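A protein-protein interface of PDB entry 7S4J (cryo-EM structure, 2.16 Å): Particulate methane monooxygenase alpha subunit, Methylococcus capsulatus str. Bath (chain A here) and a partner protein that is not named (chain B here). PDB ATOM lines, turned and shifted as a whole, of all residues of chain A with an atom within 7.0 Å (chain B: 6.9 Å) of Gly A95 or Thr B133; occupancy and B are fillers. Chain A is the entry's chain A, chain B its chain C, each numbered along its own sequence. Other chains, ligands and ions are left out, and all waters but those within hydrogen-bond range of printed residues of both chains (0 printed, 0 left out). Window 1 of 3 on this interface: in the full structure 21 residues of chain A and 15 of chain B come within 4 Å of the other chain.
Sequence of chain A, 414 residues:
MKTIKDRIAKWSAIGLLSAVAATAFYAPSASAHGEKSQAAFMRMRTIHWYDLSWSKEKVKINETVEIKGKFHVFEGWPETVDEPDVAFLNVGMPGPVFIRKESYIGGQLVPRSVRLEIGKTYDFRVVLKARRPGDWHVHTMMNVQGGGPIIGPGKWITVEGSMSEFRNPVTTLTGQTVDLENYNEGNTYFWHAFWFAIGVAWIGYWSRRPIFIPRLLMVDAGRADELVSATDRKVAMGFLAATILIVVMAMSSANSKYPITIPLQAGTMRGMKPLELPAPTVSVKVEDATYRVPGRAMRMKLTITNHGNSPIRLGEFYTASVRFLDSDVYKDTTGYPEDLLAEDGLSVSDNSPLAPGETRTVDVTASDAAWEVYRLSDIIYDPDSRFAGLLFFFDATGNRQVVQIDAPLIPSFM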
ATOM      1  N   VAL A  91      11.151  31.637 -10.794  1.00  0.00           N
ATOM      2  CA  VAL A  91       9.999  32.446 -10.425  1.00  0.00           C
ATOM      3  C   VAL A  91      10.123  32.804  -8.952  1.00  0.00           C
ATOM      4  O   VAL A  91      10.402  31.934  -8.121  1.00  0.00           O
ATOM      5  CB  VAL A  91       8.669  31.715 -10.693  1.00  0.00           C
ATOM      6  CG1 VAL A  91       7.506  32.647 -10.457  1.00  0.00           C
ATOM      7  CG2 VAL A  91       8.631  31.175 -12.107  1.00  0.00           C
ATOM      8  N   GLY A  92       9.935  34.079  -8.634  1.00  0.00           N
ATOM      9  CA  GLY A  92       9.950  34.522  -7.255  1.00  0.00           C
ATOM     10  C   GLY A  92       8.581  34.463  -6.613  1.00  0.00           C
ATOM     11  O   GLY A  92       7.677  35.200  -7.005  1.00  0.00           O
ATOM     12  N   MET A  93       8.417  33.588  -5.630  1.00  0.00           N
ATOM     13  CA  MET A  93       7.143  33.390  -4.957  1.00  0.00           C
ATOM     14  C   MET A  93       7.416  32.760  -3.602  1.00  0.00           C
ATOM     15  O   MET A  93       8.465  32.139  -3.403  1.00  0.00           O
ATOM     16  CB  MET A  93       6.206  32.502  -5.787  1.00  0.00           C
ATOM     17  CG  MET A  93       6.795  31.155  -6.149  1.00  0.00           C
ATOM     18  SD  MET A  93       5.695  30.180  -7.185  1.00  0.00           S
ATOM     19  CE  MET A  93       5.016  31.469  -8.214  1.00  0.00           C
ATOM     20  N   PRO A  94       6.493  32.901  -2.643  1.00  0.00           N
ATOM     21  CA  PRO A  94       6.723  32.311  -1.317  1.00  0.00           C
ATOM     22  C   PRO A  94       6.444  30.819  -1.297  1.00  0.00           C
ATOM     23  O   PRO A  94       5.397  30.388  -0.809  1.00  0.00           O
ATOM     24  CB  PRO A  94       5.741  33.070  -0.413  1.00  0.00           C
ATOM     25  CG  PRO A  94       5.064  34.082  -1.285  1.00  0.00           C
ATOM     26  CD  PRO A  94       5.222  33.634  -2.690  1.00  0.00           C
ATOM     27  N   GLY A  95       7.371  30.023  -1.814  1.00  0.00           N
ATOM     28  CA  GLY A  95       7.154  28.603  -1.938  1.00  0.00           C
ATOM     29  C   GLY A  95       6.223  28.293  -3.091  1.00  0.00           C
ATOM     30  O   GLY A  95       5.840  29.177  -3.858  1.00  0.00           O
ATOM     31  N   PRO A  96       5.825  27.037  -3.224  1.00  0.00           N
ATOM     32  CA  PRO A  96       4.995  26.624  -4.368  1.00  0.00           C
ATOM     33  C   PRO A  96       3.519  26.992  -4.204  1.00  0.00           C
ATOM     34  O   PRO A  96       2.638  26.131  -4.205  1.00  0.00           O
ATOM     35  CB  PRO A  96       5.210  25.105  -4.404  1.00  0.00           C
ATOM     36  CG  PRO A  96       6.134  24.770  -3.274  1.00  0.00           C
ATOM     37  CD  PRO A  96       6.129  25.908  -2.338  1.00  0.00           C
ATOM     38  N   VAL A  97       3.244  28.288  -4.057  1.00  0.00           N
ATOM     39  CA  VAL A  97       1.862  28.749  -4.159  1.00  0.00           C
ATOM     40  C   VAL A  97       1.357  28.624  -5.588  1.00  0.00           C
ATOM     41  O   VAL A  97       0.144  28.542  -5.810  1.00  0.00           O
ATOM     42  CB  VAL A  97       1.713  30.195  -3.655  1.00  0.00           C
ATOM     43  CG1 VAL A  97       2.106  30.281  -2.199  1.00  0.00           C
ATOM     44  CG2 VAL A  97       2.544  31.154  -4.493  1.00  0.00           C
ATOM     45  N   PHE A  98       2.265  28.611  -6.557  1.00  0.00           N
ATOM     46  CA  PHE A  98       2.006  28.224  -7.934  1.00  0.00           C
ATOM     47  C   PHE A  98       2.955  27.081  -8.242  1.00  0.00           C
ATOM     48  O   PHE A  98       3.984  26.938  -7.576  1.00  0.00           O
ATOM     49  CB  PHE A  98       2.269  29.376  -8.907  1.00  0.00           C
ATOM     50  CG  PHE A  98       1.255  30.476  -8.859  1.00  0.00           C
ATOM     51  CD1 PHE A  98       1.419  31.543  -7.995  1.00  0.00           C
ATOM     52  CD2 PHE A  98       0.151  30.455  -9.684  1.00  0.00           C
ATOM     53  CE1 PHE A  98       0.496  32.559  -7.955  1.00  0.00           C
ATOM     54  CE2 PHE A  98      -0.771  31.471  -9.648  1.00  0.00           C
ATOM     55  CZ  PHE A  98      -0.599  32.522  -8.784  1.00  0.00           C
ATOM     56  N   ILE A  99       2.629  26.275  -9.235  1.00  0.00           N
ATOM     57  CA  ILE A  99       3.600  25.350  -9.798  1.00  0.00           C
ATOM     58  C   ILE A  99       3.970  25.837 -11.190  1.00  0.00           C
ATOM     59  O   ILE A  99       3.113  26.308 -11.944  1.00  0.00           O
ATOM     60  CB  ILE A  99       3.064  23.910  -9.830  1.00  0.00           C
ATOM     61  CG1 ILE A  99       1.766  23.816 -10.627  1.00  0.00           C
ATOM     62  CG2 ILE A  99       2.885  23.378  -8.421  1.00  0.00           C
ATOM     63  CD1 ILE A  99       1.629  22.521 -11.374  1.00  0.00           C
ATOM     64  N   ARG A 131      -1.991  26.984  -7.076  1.00  0.00           N
ATOM     65  CA  ARG A 131      -1.998  25.868  -6.137  1.00  0.00           C
ATOM     66  C   ARG A 131      -2.511  26.235  -4.754  1.00  0.00           C
ATOM     67  O   ARG A 131      -3.240  25.449  -4.151  1.00  0.00           O
ATOM     68  CB  ARG A 131      -0.584  25.281  -6.026  1.00  0.00           C
ATOM     69  CG  ARG A 131      -0.488  24.030  -5.177  1.00  0.00           C
ATOM     70  CD  ARG A 131       0.895  23.428  -5.270  1.00  0.00           C
ATOM     71  NE  ARG A 131       1.094  22.329  -4.338  1.00  0.00           N
ATOM     72  CZ  ARG A 131       1.791  22.420  -3.215  1.00  0.00           C
ATOM     73  NH1 ARG A 131       2.345  23.558  -2.836  1.00  0.00           N
ATOM     74  NH2 ARG A 131       1.937  21.341  -2.453  1.00  0.00           N
ATOM     75  N   ARG A 132      -2.156  27.406  -4.236  1.00  0.00           N
ATOM     76  CA  ARG A 132      -2.485  27.782  -2.875  1.00  0.00           C
ATOM     77  C   ARG A 132      -3.272  29.085  -2.862  1.00  0.00           C
ATOM     78  O   ARG A 132      -2.841  30.068  -3.478  1.00  0.00           O
ATOM     79  CB  ARG A 132      -1.216  27.941  -2.036  1.00  0.00           C
ATOM     80  CG  ARG A 132      -0.817  26.701  -1.272  1.00  0.00           C
ATOM     81  CD  ARG A 132       0.341  26.997  -0.345  1.00  0.00           C
ATOM     82  NE  ARG A 132      -0.101  27.692   0.857  1.00  0.00           N
ATOM     83  CZ  ARG A 132       0.616  28.595   1.506  1.00  0.00           C
ATOM     84  NH1 ARG A 132       1.824  28.942   1.099  1.00  0.00           N
ATOM     85  NH2 ARG A 132       0.110  29.162   2.595  1.00  0.00           N
ATOM     86  N   TRP B  45       4.428  34.648   6.420  1.00  0.00           N
ATOM     87  CA  TRP B  45       3.845  35.536   5.429  1.00  0.00           C
ATOM     88  C   TRP B  45       2.941  36.519   6.148  1.00  0.00           C
ATOM     89  O   TRP B  45       2.618  36.331   7.324  1.00  0.00           O
ATOM     90  CB  TRP B  45       3.051  34.756   4.379  1.00  0.00           C
ATOM     91  CG  TRP B  45       3.673  33.455   3.968  1.00  0.00           C
ATOM     92  CD1 TRP B  45       4.372  33.203   2.825  1.00  0.00           C
ATOM     93  CD2 TRP B  45       3.640  32.226   4.696  1.00  0.00           C
ATOM     94  NE1 TRP B  45       4.781  31.893   2.798  1.00  0.00           N
ATOM     95  CE2 TRP B  45       4.344  31.273   3.938  1.00  0.00           C
ATOM     96  CE3 TRP B  45       3.086  31.841   5.917  1.00  0.00           C
ATOM     97  CZ2 TRP B  45       4.508  29.964   4.362  1.00  0.00           C
ATOM     98  CZ3 TRP B  45       3.249  30.545   6.336  1.00  0.00           C
ATOM     99  CH2 TRP B  45       3.951  29.622   5.561  1.00  0.00           C
ATOM    100  N   GLY B 128      16.325  26.179   6.951  1.00  0.00           N
ATOM    101  CA  GLY B 128      16.561  25.553   5.634  1.00  0.00           C
ATOM    102  C   GLY B 128      15.340  25.616   4.734  1.00  0.00           C
ATOM    103  O   GLY B 128      15.503  26.049   3.593  1.00  0.00           O
ATOM    104  N   THR B 129      14.157  25.219   5.224  1.00  0.00           N
ATOM    105  CA  THR B 129      12.903  25.317   4.418  1.00  0.00           C
ATOM    106  C   THR B 129      12.760  26.742   3.869  1.00  0.00           C
ATOM    107  O   THR B 129      12.498  26.876   2.659  1.00  0.00           O
ATOM    108  CB  THR B 129      11.651  24.882   5.201  1.00  0.00           C
ATOM    109  OG1 THR B 129      10.922  26.013   5.685  1.00  0.00           O
ATOM    110  CG2 THR B 129      11.965  23.984   6.374  1.00  0.00           C
ATOM    111  N   TRP B 130      12.941  27.753   4.725  1.00  0.00           N
ATOM    112  CA  TRP B 130      12.815  29.174   4.306  1.00  0.00           C
ATOM    113  C   TRP B 130      13.850  29.511   3.225  1.00  0.00           C
ATOM    114  O   TRP B 130      13.533  30.351   2.373  1.00  0.00           O
ATOM    115  CB  TRP B 130      12.946  30.083   5.535  1.00  0.00           C
ATOM    116  CG  TRP B 130      12.030  31.269   5.561  1.00  0.00           C
ATOM    117  CD1 TRP B 130      12.395  32.566   5.774  1.00  0.00           C
ATOM    118  CD2 TRP B 130      10.598  31.280   5.397  1.00  0.00           C
ATOM    119  NE1 TRP B 130      11.300  33.384   5.742  1.00  0.00           N
ATOM    120  CE2 TRP B 130      10.183  32.625   5.515  1.00  0.00           C
ATOM    121  CE3 TRP B 130       9.627  30.300   5.160  1.00  0.00           C
ATOM    122  CZ2 TRP B 130       8.846  33.005   5.404  1.00  0.00           C
ATOM    123  CZ3 TRP B 130       8.306  30.677   5.050  1.00  0.00           C
ATOM    124  CH2 TRP B 130       7.923  32.012   5.170  1.00  0.00           C
ATOM    125  N   HIS B 131      15.003  28.834   3.209  1.00  0.00           N
ATOM    126  CA  HIS B 131      16.101  29.162   2.251  1.00  0.00           C
ATOM    127  C   HIS B 131      15.763  28.763   0.814  1.00  0.00           C
ATOM    128  O   HIS B 131      16.471  29.222  -0.095  1.00  0.00           O
ATOM    129  CB  HIS B 131      17.428  28.581   2.770  1.00  0.00           C
ATOM    130  CG  HIS B 131      17.878  29.458   3.875  1.00  0.00           C
ATOM    131  ND1 HIS B 131      17.194  30.636   4.061  1.00  0.00           N
ATOM    132  CD2 HIS B 131      18.830  29.368   4.842  1.00  0.00           C
ATOM    133  CE1 HIS B 131      17.713  31.263   5.042  1.00  0.00           C
ATOM    134  NE2 HIS B 131      18.710  30.519   5.567  1.00  0.00           N
ATOM    135  N   GLN B 132      14.718  27.960   0.627  1.00  0.00           N
ATOM    136  CA  GLN B 132      14.346  27.491  -0.728  1.00  0.00           C
ATOM    137  C   GLN B 132      12.953  28.026  -1.070  1.00  0.00           C
ATOM    138  O   GLN B 132      12.265  27.392  -1.888  1.00  0.00           O
ATOM    139  CB  GLN B 132      14.446  25.967  -0.745  1.00  0.00           C
ATOM    140  CG  GLN B 132      15.859  25.475  -0.462  1.00  0.00           C
ATOM    141  CD  GLN B 132      16.037  24.778   0.862  1.00  0.00           C
ATOM    142  OE1 GLN B 132      15.123  24.143   1.385  1.00  0.00           O
ATOM    143  NE2 GLN B 132      17.229  24.894   1.422  1.00  0.00           N
ATOM    144  N   THR B 133      12.556  29.147  -0.455  1.00  0.00           N
ATOM    145  CA  THR B 133      11.218  29.746  -0.705  1.00  0.00           C
ATOM    146  C   THR B 133      11.337  31.261  -0.859  1.00  0.00           C
ATOM    147  O   THR B 133      10.512  31.837  -1.571  1.00  0.00           O
ATOM    148  CB  THR B 133      10.234  29.452   0.434  1.00  0.00           C
ATOM    149  OG1 THR B 133      10.734  30.003   1.653  1.00  0.00           O
ATOM    150  CG2 THR B 133       9.983  27.974   0.608  1.00  0.00           C
ATOM    151  N   ILE B 134      12.303  31.881  -0.182  1.00  0.00           N
ATOM    152  CA  ILE B 134      12.420  33.329  -0.233  1.00  0.00           C
ATOM    153  C   ILE B 134      13.770  33.703  -0.827  1.00  0.00           C
ATOM    154  O   ILE B 134      14.625  32.856  -1.082  1.00  0.00           O
ATOM    155  CB  ILE B 134      12.201  33.988   1.153  1.00  0.00           C
ATOM    156  CG1 ILE B 134      13.166  33.485   2.249  1.00  0.00           C
ATOM    157  CG2 ILE B 134      10.763  33.799   1.609  1.00  0.00           C
ATOM    158  CD1 ILE B 134      14.661  33.751   2.089  1.00  0.00           C
ATOM    159  N   VAL B 135      13.943  34.999  -1.047  1.00  0.00           N
ATOM    160  CA  VAL B 135      15.243  35.601  -1.301  1.00  0.00           C
ATOM    161  C   VAL B 135      15.542  36.482  -0.096  1.00  0.00           C
ATOM    162  O   VAL B 135      14.722  37.335   0.268  1.00  0.00           O
ATOM    163  CB  VAL B 135      15.256  36.409  -2.609  1.00  0.00           C
ATOM    164  CG1 VAL B 135      16.528  37.214  -2.723  1.00  0.00           C
ATOM    165  CG2 VAL B 135      15.100  35.489  -3.803  1.00  0.00           C
ATOM    166  N   GLU B 209      22.121  29.505  -2.371  1.00  0.00           N
ATOM    167  CA  GLU B 209      21.529  29.056  -1.107  1.00  0.00           C
ATOM    168  C   GLU B 209      21.940  27.629  -0.770  1.00  0.00           C
ATOM    169  O   GLU B 209      21.134  26.897  -0.188  1.00  0.00           O
ATOM    170  CB  GLU B 209      20.005  29.177  -1.158  1.00  0.00           C
ATOM    171  CG  GLU B 209      19.509  30.609  -1.229  1.00  0.00           C
ATOM    172  CD  GLU B 209      19.319  31.233   0.138  1.00  0.00           C
ATOM    173  OE1 GLU B 209      20.163  31.000   1.030  1.00  0.00           O
ATOM    174  OE2 GLU B 209      18.324  31.965   0.320  1.00  0.00           O
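Thr B133 touches just these residues of chain A: Met A93, Pro A94 and Gly A95. Of the printed residues of chain B, Pro A94 touches Trp B45 and Thr B133. Printed residues of chain A within 4 Å of Trp B45: Pro A94 (3.5 Å). Of the printed residues of chain B, Met A93 touches Thr B133. Val A91 touches none of the printed residues of chain B.
OG1 of Thr B133 is in hydrogen-bond range of O of Trp B130 (2.9 Å).
Among the printed residues, pairs that only touch across the chains: Pro A94 with Trp B45 (3.5 Å), Pro A94 with Thr B133 (3.8 Å) and Gly A95 with Thr B133 (3.6 Å).
The backbone carbonyl oxygen (O) of Thr B133 sits close to the backbone carbonyl oxygen (O) of Met A93.
Of the 10 printed residues of chain B, 2 touch a printed residue of chain A. Hydrophobic or aromatic side chains of chain B within 4 Å of the printed part of chain A: Trp B45. Along chain A the printed residues that touch a printed residue of chain B span positions 93 to 95. Among the printed residues, 4 pairs touch across the chains. Among the printed residues, no Asp or Glu carboxylate lies within 4 Å of a Lys or Arg side-chain nitrogen of the other chain.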
